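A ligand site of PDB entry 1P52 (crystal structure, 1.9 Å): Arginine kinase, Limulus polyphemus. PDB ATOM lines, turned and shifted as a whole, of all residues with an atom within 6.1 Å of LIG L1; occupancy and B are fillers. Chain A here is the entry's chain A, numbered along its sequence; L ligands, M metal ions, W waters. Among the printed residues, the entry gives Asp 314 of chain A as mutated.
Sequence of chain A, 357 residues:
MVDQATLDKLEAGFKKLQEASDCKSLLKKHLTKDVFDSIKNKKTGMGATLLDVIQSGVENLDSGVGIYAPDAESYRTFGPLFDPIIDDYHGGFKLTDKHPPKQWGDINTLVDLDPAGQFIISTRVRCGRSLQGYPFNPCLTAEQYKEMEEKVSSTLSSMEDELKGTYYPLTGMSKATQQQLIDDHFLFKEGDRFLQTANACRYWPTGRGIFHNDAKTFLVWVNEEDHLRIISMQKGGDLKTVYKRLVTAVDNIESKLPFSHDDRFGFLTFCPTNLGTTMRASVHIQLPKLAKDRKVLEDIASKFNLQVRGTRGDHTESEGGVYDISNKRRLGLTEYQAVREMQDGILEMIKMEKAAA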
ATOM      1  N   SER A  25      17.009 -32.308 -31.645  1.00  0.00           N
ATOM      2  CA  SER A  25      16.798 -30.906 -32.017  1.00  0.00           C
ATOM      3  C   SER A  25      15.737 -30.736 -33.102  1.00  0.00           C
ATOM      4  O   SER A  25      15.525 -31.631 -33.928  1.00  0.00           O
ATOM      5  CB  SER A  25      18.104 -30.292 -32.512  1.00  0.00           C
ATOM      6  OG  SER A  25      18.441 -30.789 -33.798  1.00  0.00           O
ATOM      7  N   SER A  56      25.312 -24.130 -36.244  1.00  0.00           N
ATOM      8  CA  SER A  56      25.309 -24.310 -34.789  1.00  0.00           C
ATOM      9  C   SER A  56      24.660 -25.630 -34.403  1.00  0.00           C
ATOM     10  O   SER A  56      25.149 -26.337 -33.508  1.00  0.00           O
ATOM     11  CB  SER A  56      24.579 -23.153 -34.104  1.00  0.00           C
ATOM     12  OG  SER A  56      24.679 -23.272 -32.700  1.00  0.00           O
ATOM     13  N   ASP A  62      23.399 -31.518 -29.287  1.00  0.00           N
ATOM     14  CA  ASP A  62      22.560 -31.394 -28.102  1.00  0.00           C
ATOM     15  C   ASP A  62      21.679 -30.150 -28.152  1.00  0.00           C
ATOM     16  O   ASP A  62      21.019 -29.820 -27.173  1.00  0.00           O
ATOM     17  CB  ASP A  62      23.430 -31.411 -26.838  1.00  0.00           C
ATOM     18  CG  ASP A  62      24.492 -30.340 -26.861  1.00  0.00           C
ATOM     19  OD1 ASP A  62      24.853 -29.868 -27.959  1.00  0.00           O
ATOM     20  OD2 ASP A  62      24.953 -29.982 -25.759  1.00  0.00           O
ATOM     21  N   SER A  63      21.692 -29.468 -29.286  1.00  0.00           N
ATOM     22  CA  SER A  63      20.870 -28.267 -29.476  1.00  0.00           C
ATOM     23  C   SER A  63      19.407 -28.663 -29.349  1.00  0.00           C
ATOM     24  O   SER A  63      19.030 -29.776 -29.703  1.00  0.00           O
ATOM     25  CB  SER A  63      21.091 -27.679 -30.868  1.00  0.00           C
ATOM     26  OG  SER A  63      22.360 -27.056 -31.000  1.00  0.00           O
ATOM     27  N   GLY A  64      18.583 -27.743 -28.855  1.00  0.00           N
ATOM     28  CA  GLY A  64      17.163 -28.035 -28.746  1.00  0.00           C
ATOM     29  C   GLY A  64      16.479 -27.579 -30.029  1.00  0.00           C
ATOM     30  O   GLY A  64      15.538 -28.200 -30.525  1.00  0.00           O
ATOM     31  N   VAL A  65      16.985 -26.474 -30.571  1.00  0.00           N
ATOM     32  CA  VAL A  65      16.455 -25.884 -31.787  1.00  0.00           C
ATOM     33  C   VAL A  65      17.473 -26.073 -32.905  1.00  0.00           C
ATOM     34  O   VAL A  65      17.206 -26.758 -33.892  1.00  0.00           O
ATOM     35  CB  VAL A  65      16.150 -24.393 -31.557  1.00  0.00           C
ATOM     36  CG1 VAL A  65      15.620 -23.752 -32.840  1.00  0.00           C
ATOM     37  CG2 VAL A  65      15.133 -24.264 -30.421  1.00  0.00           C
ATOM     38  N   GLY A  66      18.652 -25.461 -32.761  1.00  0.00           N
ATOM     39  CA  GLY A  66      19.695 -25.644 -33.751  1.00  0.00           C
ATOM     40  C   GLY A  66      19.898 -24.666 -34.898  1.00  0.00           C
ATOM     41  O   GLY A  66      20.824 -24.859 -35.690  1.00  0.00           O
ATOM     42  N   ILE A  67      19.074 -23.640 -35.008  1.00  0.00           N
ATOM     43  CA  ILE A  67      19.272 -22.705 -36.108  1.00  0.00           C
ATOM     44  C   ILE A  67      19.145 -21.260 -35.627  1.00  0.00           C
ATOM     45  O   ILE A  67      18.549 -21.006 -34.591  1.00  0.00           O
ATOM     46  CB  ILE A  67      18.258 -22.939 -37.252  1.00  0.00           C
ATOM     47  CG1 ILE A  67      16.871 -22.469 -36.837  1.00  0.00           C
ATOM     48  CG2 ILE A  67      18.209 -24.429 -37.608  1.00  0.00           C
ATOM     49  CD1 ILE A  67      15.849 -22.546 -37.924  1.00  0.00           C
ATOM     50  N   TYR A  68      19.702 -20.348 -36.415  1.00  0.00           N
ATOM     51  CA  TYR A  68      19.647 -18.916 -36.140  1.00  0.00           C
ATOM     52  C   TYR A  68      19.484 -18.182 -37.466  1.00  0.00           C
ATOM     53  O   TYR A  68      19.775 -18.740 -38.523  1.00  0.00           O
ATOM     54  CB  TYR A  68      20.946 -18.442 -35.488  1.00  0.00           C
ATOM     55  CG  TYR A  68      21.213 -18.972 -34.103  1.00  0.00           C
ATOM     56  CD1 TYR A  68      21.925 -20.157 -33.910  1.00  0.00           C
ATOM     57  CD2 TYR A  68      20.792 -18.244 -32.979  1.00  0.00           C
ATOM     58  CE1 TYR A  68      22.227 -20.603 -32.612  1.00  0.00           C
ATOM     59  CE2 TYR A  68      21.082 -18.696 -31.686  1.00  0.00           C
ATOM     60  CZ  TYR A  68      21.806 -19.871 -31.512  1.00  0.00           C
ATOM     61  OH  TYR A  68      22.102 -20.294 -30.232  1.00  0.00           O
ATOM     62  N   ARG A 126      12.344 -10.209 -19.318  1.00  0.00           N
ATOM     63  CA  ARG A 126      13.178  -9.532 -20.300  1.00  0.00           C
ATOM     64  C   ARG A 126      12.550  -9.548 -21.668  1.00  0.00           C
ATOM     65  O   ARG A 126      11.692 -10.392 -21.952  1.00  0.00           O
ATOM     66  CB  ARG A 126      14.583 -10.169 -20.407  1.00  0.00           C
ATOM     67  CG  ARG A 126      14.664 -11.651 -20.836  1.00  0.00           C
ATOM     68  CD  ARG A 126      14.553 -11.881 -22.364  1.00  0.00           C
ATOM     69  NE  ARG A 126      15.071 -13.208 -22.743  1.00  0.00           N
ATOM     70  CZ  ARG A 126      14.767 -13.863 -23.859  1.00  0.00           C
ATOM     71  NH1 ARG A 126      15.303 -15.058 -24.093  1.00  0.00           N
ATOM     72  NH2 ARG A 126      13.916 -13.344 -24.748  1.00  0.00           N
ATOM     73  N   PHE A 194      26.863 -22.624 -28.485  1.00  0.00           N
ATOM     74  CA  PHE A 194      25.803 -22.542 -29.495  1.00  0.00           C
ATOM     75  C   PHE A 194      25.915 -21.211 -30.258  1.00  0.00           C
ATOM     76  O   PHE A 194      25.848 -21.192 -31.489  1.00  0.00           O
ATOM     77  CB  PHE A 194      24.420 -22.667 -28.840  1.00  0.00           C
ATOM     78  CG  PHE A 194      24.263 -23.929 -28.016  1.00  0.00           C
ATOM     79  CD1 PHE A 194      24.550 -23.927 -26.652  1.00  0.00           C
ATOM     80  CD2 PHE A 194      23.911 -25.121 -28.634  1.00  0.00           C
ATOM     81  CE1 PHE A 194      24.496 -25.102 -25.913  1.00  0.00           C
ATOM     82  CE2 PHE A 194      23.846 -26.317 -27.902  1.00  0.00           C
ATOM     83  CZ  PHE A 194      24.145 -26.300 -26.544  1.00  0.00           C
ATOM     84  N   LEU A 195      26.135 -20.117 -29.536  1.00  0.00           N
ATOM     85  CA  LEU A 195      26.273 -18.814 -30.187  1.00  0.00           C
ATOM     86  C   LEU A 195      27.569 -18.723 -30.993  1.00  0.00           C
ATOM     87  O   LEU A 195      27.605 -18.193 -32.109  1.00  0.00           O
ATOM     88  CB  LEU A 195      26.242 -17.678 -29.150  1.00  0.00           C
ATOM     89  CG  LEU A 195      24.877 -17.323 -28.556  1.00  0.00           C
ATOM     90  CD1 LEU A 195      25.051 -16.238 -27.504  1.00  0.00           C
ATOM     91  CD2 LEU A 195      23.927 -16.858 -29.673  1.00  0.00           C
ATOM     92  N   GLU A 225      23.451 -11.902 -27.590  1.00  0.00           N
ATOM     93  CA  GLU A 225      22.720 -12.653 -28.611  1.00  0.00           C
ATOM     94  C   GLU A 225      21.918 -11.748 -29.543  1.00  0.00           C
ATOM     95  O   GLU A 225      21.889 -11.957 -30.762  1.00  0.00           O
ATOM     96  CB  GLU A 225      21.814 -13.698 -27.955  1.00  0.00           C
ATOM     97  CG  GLU A 225      20.925 -14.445 -28.956  1.00  0.00           C
ATOM     98  CD  GLU A 225      20.168 -15.589 -28.312  1.00  0.00           C
ATOM     99  OE1 GLU A 225      19.059 -15.904 -28.798  1.00  0.00           O
ATOM    100  OE2 GLU A 225      20.689 -16.175 -27.342  1.00  0.00           O
ATOM    101  N   ARG A 229      18.930  -6.483 -24.913  1.00  0.00           N
ATOM    102  CA  ARG A 229      18.073  -7.328 -24.076  1.00  0.00           C
ATOM    103  C   ARG A 229      17.751  -6.355 -22.934  1.00  0.00           C
ATOM    104  O   ARG A 229      18.672  -5.850 -22.268  1.00  0.00           O
ATOM    105  CB  ARG A 229      18.782  -8.591 -23.552  1.00  0.00           C
ATOM    106  CG  ARG A 229      19.020  -9.710 -24.592  1.00  0.00           C
ATOM    107  CD  ARG A 229      17.693 -10.245 -25.220  1.00  0.00           C
ATOM    108  NE  ARG A 229      17.904 -11.374 -26.135  1.00  0.00           N
ATOM    109  CZ  ARG A 229      18.200 -12.616 -25.756  1.00  0.00           C
ATOM    110  NH1 ARG A 229      18.311 -12.904 -24.472  1.00  0.00           N
ATOM    111  NH2 ARG A 229      18.364 -13.591 -26.660  1.00  0.00           N
ATOM    112  N   CYS A 271      17.451 -15.462 -32.746  1.00  0.00           N
ATOM    113  CA  CYS A 271      16.964 -16.827 -32.617  1.00  0.00           C
ATOM    114  C   CYS A 271      15.451 -16.848 -32.818  1.00  0.00           C
ATOM    115  O   CYS A 271      14.728 -15.982 -32.311  1.00  0.00           O
ATOM    116  CB  CYS A 271      17.286 -17.411 -31.238  1.00  0.00           C
ATOM    117  SG  CYS A 271      16.633 -19.109 -30.971  1.00  0.00           S
ATOM    118  N   THR A 273      13.323 -18.594 -31.465  1.00  0.00           N
ATOM    119  CA  THR A 273      12.592 -18.767 -30.212  1.00  0.00           C
ATOM    120  C   THR A 273      12.232 -17.439 -29.564  1.00  0.00           C
ATOM    121  O   THR A 273      11.322 -17.372 -28.734  1.00  0.00           O
ATOM    122  CB  THR A 273      13.419 -19.565 -29.154  1.00  0.00           C
ATOM    123  OG1 THR A 273      14.561 -18.799 -28.777  1.00  0.00           O
ATOM    124  CG2 THR A 273      13.851 -20.904 -29.694  1.00  0.00           C
ATOM    125  N   ASN A 274      12.931 -16.368 -29.935  1.00  0.00           N
ATOM    126  CA  ASN A 274      12.690 -15.056 -29.344  1.00  0.00           C
ATOM    127  C   ASN A 274      11.872 -14.029 -30.120  1.00  0.00           C
ATOM    128  O   ASN A 274      11.782 -12.872 -29.717  1.00  0.00           O
ATOM    129  CB  ASN A 274      14.033 -14.440 -28.948  1.00  0.00           C
ATOM    130  CG  ASN A 274      14.663 -15.175 -27.789  1.00  0.00           C
ATOM    131  OD1 ASN A 274      13.988 -15.480 -26.815  1.00  0.00           O
ATOM    132  ND2 ASN A 274      15.951 -15.482 -27.893  1.00  0.00           N
ATOM    133  N   ARG A 309      15.244 -24.459 -17.099  1.00  0.00           N
ATOM    134  CA  ARG A 309      16.664 -24.264 -17.398  1.00  0.00           C
ATOM    135  C   ARG A 309      17.419 -24.348 -16.089  1.00  0.00           C
ATOM    136  O   ARG A 309      16.814 -24.320 -15.020  1.00  0.00           O
ATOM    137  CB  ARG A 309      16.918 -22.875 -18.009  1.00  0.00           C
ATOM    138  CG  ARG A 309      16.227 -22.645 -19.322  1.00  0.00           C
ATOM    139  CD  ARG A 309      16.447 -21.223 -19.810  1.00  0.00           C
ATOM    140  NE  ARG A 309      15.792 -21.064 -21.106  1.00  0.00           N
ATOM    141  CZ  ARG A 309      16.115 -20.123 -21.988  1.00  0.00           C
ATOM    142  NH1 ARG A 309      17.076 -19.252 -21.710  1.00  0.00           N
ATOM    143  NH2 ARG A 309      15.496 -20.099 -23.164  1.00  0.00           N
ATOM    144  N   ASP A 314      20.394 -21.040 -19.973  1.00  0.00           N
ATOM    145  CA  ASP A 314      20.396 -21.941 -21.123  1.00  0.00           C
ATOM    146  C   ASP A 314      21.448 -23.059 -20.994  1.00  0.00           C
ATOM    147  O   ASP A 314      22.620 -22.772 -20.769  1.00  0.00           O
ATOM    148  CB  ASP A 314      20.769 -21.089 -22.348  1.00  0.00           C
ATOM    149  CG  ASP A 314      19.877 -21.311 -23.536  1.00  0.00           C
ATOM    150  OD1 ASP A 314      18.992 -22.191 -23.492  1.00  0.00           O
ATOM    151  OD2 ASP A 314      20.090 -20.561 -24.520  1.00  0.00           O
ATOM    152  N   HIS A 315      21.048 -24.310 -21.177  1.00  0.00           N
ATOM    153  CA  HIS A 315      21.977 -25.437 -21.135  1.00  0.00           C
ATOM    154  C   HIS A 315      22.882 -25.574 -19.919  1.00  0.00           C
ATOM    155  O   HIS A 315      24.046 -25.964 -20.033  1.00  0.00           O
ATOM    156  CB  HIS A 315      22.843 -25.448 -22.412  1.00  0.00           C
ATOM    157  CG  HIS A 315      22.077 -25.707 -23.663  1.00  0.00           C
ATOM    158  ND1 HIS A 315      21.727 -24.709 -24.548  1.00  0.00           N
ATOM    159  CD2 HIS A 315      21.545 -26.851 -24.157  1.00  0.00           C
ATOM    160  CE1 HIS A 315      21.008 -25.236 -25.532  1.00  0.00           C
ATOM    161  NE2 HIS A 315      20.884 -26.533 -25.313  1.00  0.00           N
HETATM  162  N1  LIG L   1      20.700 -22.718 -30.177  1.00  0.00           N
HETATM  163  C1  LIG L   1      20.436 -23.334 -28.869  1.00  0.00           C
HETATM  164  C2  LIG L   1      19.671 -22.356 -27.974  1.00  0.00           C
HETATM  165  C3  LIG L   1      18.330 -21.873 -28.528  1.00  0.00           C
HETATM  166  C4  LIG L   1      17.450 -21.226 -27.433  1.00  0.00           C
HETATM  167  N2  LIG L   1      18.228 -20.264 -26.650  1.00  0.00           N
HETATM  168  C5  LIG L   1      18.563 -19.048 -27.055  1.00  0.00           C
HETATM  169  N3  LIG L   1      18.188 -18.589 -28.254  1.00  0.00           N
HETATM  170  N4  LIG L   1      19.320 -18.288 -26.266  1.00  0.00           N
HETATM  171  C6  LIG L   1      19.642 -24.638 -28.988  1.00  0.00           C
HETATM  172  O1  LIG L   1      18.970 -24.860 -29.997  1.00  0.00           O
HETATM  173  P1  LG2 L   2      17.997 -14.954 -21.404  1.00  0.00           P
HETATM  174  O1  LG2 L   2      19.125 -14.835 -22.384  1.00  0.00           O
HETATM  175  O2  LG2 L   2      17.833 -13.676 -20.687  1.00  0.00           O
HETATM  176  O3  LG2 L   2      16.700 -15.381 -22.029  1.00  0.00           O
HETATM  177  P2  LG2 L   2      19.483 -17.128 -20.077  1.00  0.00           P
HETATM  178  O4  LG2 L   2      20.497 -17.085 -21.169  1.00  0.00           O
HETATM  179  O5  LG2 L   2      18.951 -18.453 -19.721  1.00  0.00           O
HETATM  180  O6  LG2 L   2      18.282 -16.079 -20.330  1.00  0.00           O
HETATM  181  O7  LG2 L   2      20.093 -16.551 -18.690  1.00  0.00           O
HETATM  182  C1  LG2 L   2      20.841 -15.354 -18.636  1.00  0.00           C
HETATM  183  C2  LG2 L   2      20.970 -14.944 -17.174  1.00  0.00           C
HETATM  184  O8  LG2 L   2      19.702 -14.570 -16.583  1.00  0.00           O
HETATM  185  C3  LG2 L   2      21.527 -16.058 -16.305  1.00  0.00           C
HETATM  186  O9  LG2 L   2      22.520 -15.467 -15.449  1.00  0.00           O
HETATM  187  C4  LG2 L   2      20.366 -16.526 -15.458  1.00  0.00           C
HETATM  188  O10 LG2 L   2      20.749 -17.102 -14.178  1.00  0.00           O
HETATM  189  C5  LG2 L   2      19.563 -15.239 -15.315  1.00  0.00           C
HETATM  190  N1  LG2 L   2      18.141 -15.472 -14.885  1.00  0.00           N
HETATM  191  C6  LG2 L   2      17.085 -15.890 -15.610  1.00  0.00           C
HETATM  192  N2  LG2 L   2      15.983 -15.894 -14.852  1.00  0.00           N
HETATM  193  C7  LG2 L   2      16.368 -15.446 -13.654  1.00  0.00           C
HETATM  194  C8  LG2 L   2      15.531 -15.152 -12.562  1.00  0.00           C
HETATM  195  N3  LG2 L   2      14.215 -15.420 -12.496  1.00  0.00           N
HETATM  196  N4  LG2 L   2      16.161 -14.651 -11.473  1.00  0.00           N
HETATM  197  C9  LG2 L   2      17.476 -14.426 -11.483  1.00  0.00           C
HETATM  198  N5  LG2 L   2      18.263 -14.669 -12.537  1.00  0.00           N
HETATM  199  C10 LG2 L   2      17.716 -15.200 -13.648  1.00  0.00           C
HETATM  200 MG    MG M   1      20.588 -16.091 -22.928  1.00  0.00          MG
HETATM  201  O   HOH W   1      15.121 -23.673 -26.642  1.00  0.00           O
HETATM  202  O   HOH W   2      18.407 -21.657 -31.957  1.00  0.00           O
HETATM  203  O   HOH W   3      21.962 -18.781 -28.170  1.00  0.00           O
HETATM  204  O   HOH W   4      22.200 -24.427 -31.742  1.00  0.00           O
HETATM  205  O   HOH W   5      17.482 -24.661 -26.239  1.00  0.00           O
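Merely in contact with LIG L1: Ser 63, Thr 273, His 315, Asn 274 and Phe 194.
Hydrophobic or aromatic side chains that line LIG L1: Val 65, Tyr 68, Phe 194 and His 315.
12 residues have an atom within 4 Å of LIG L1: Ser 63, Gly 64, Val 65, Gly 66, Tyr 68, Phe 194, Glu 225, Cys 271, Thr 273, Asn 274, Asp 314 and His 315.
The guanidinium group of Arg 229 is in salt-bridge range of the side-chain carboxylate of Glu 225.
NH1 of Arg 309 is in salt-bridge range of OD1 of Asp 314 (3.9 Å).
The side-chain amide oxygen (OD1) of Asn 274 sits at hydrogen-bond distance from the guanidinium group (NH2) of Arg 126, at 3.0 Å.
The side-chain sulfur (SG) of Cys 271 lies within hydrogen-bond range of the side-chain hydroxyl (OG1) of Thr 273 (3.0 Å).
NH2 of Arg 229 lies close to ND2 of Asn 274, at 3.3 Å.
O of Phe 194 sits at hydrogen-bond distance from OG of Ser 56 (2.7 Å).
The side-chain carboxylate (OE1) of Glu 225 sits at hydrogen-bond distance from the side-chain amide nitrogen (ND2) of Asn 274.
O1 of LIG L1 sits at hydrogen-bond distance from N of Gly 64, 3.1 Å away.
An oxygen (O3) of LG2 L2 is in salt-bridge range of the guanidinium group (NH1) of Arg 229, 3.8 Å away.
The guanidinium group (NH1) of Arg 126 lies within salt-bridge range of an oxygen (O3) of LG2 L2, 2.5 Å away.
OD2 of Asp 314 lies within salt-bridge range of N2 of LIG L1 (2.8 Å).
O1 of LIG L1 is in hydrogen-bond range of N of Gly 66, 2.8 Å away.
N4 of LIG L1 is in salt-bridge range of OE2 of Glu 225 (2.7 Å).
O5 of LG2 L2 lies within salt-bridge range of NH1 of Arg 309 (2.8 Å).
The backbone NH (N) of Asp 314 is in hydrogen-bond range of an oxygen (O5) of LG2 L2 (3.0 Å).
O1 of LIG L1 lies within hydrogen-bond range of N of Val 65 (2.6 Å).
A nitrogen (N3) of LIG L1 is in hydrogen-bond range of the side-chain sulfur (SG) of Cys 271 (3.2 Å).
N1 of LIG L1 sits at hydrogen-bond distance from OH of Tyr 68 (2.8 Å).
Water W4 lies within hydrogen-bond range of the side-chain hydroxyl (OG) of Ser 63 (2.7 Å), a nitrogen (N1) of LIG L1 (2.8 Å) and the side-chain hydroxyl (OG) of Ser 56 (2.9 Å).
Water W2 lies within hydrogen-bond range of the backbone carbonyl oxygen (O) of Ile 67 (2.7 Å), a nitrogen (N1) of LIG L1 (3.1 Å) and the side-chain sulfur (SG) of Cys 271 (3.3 Å).
Water W3 lies within hydrogen-bond range of the side-chain hydroxyl of Tyr 68 (2.6 Å), the side-chain carboxylate of Glu 225 (3.0 Å) and a nitrogen (N4) of LIG L1 (3.3 Å).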
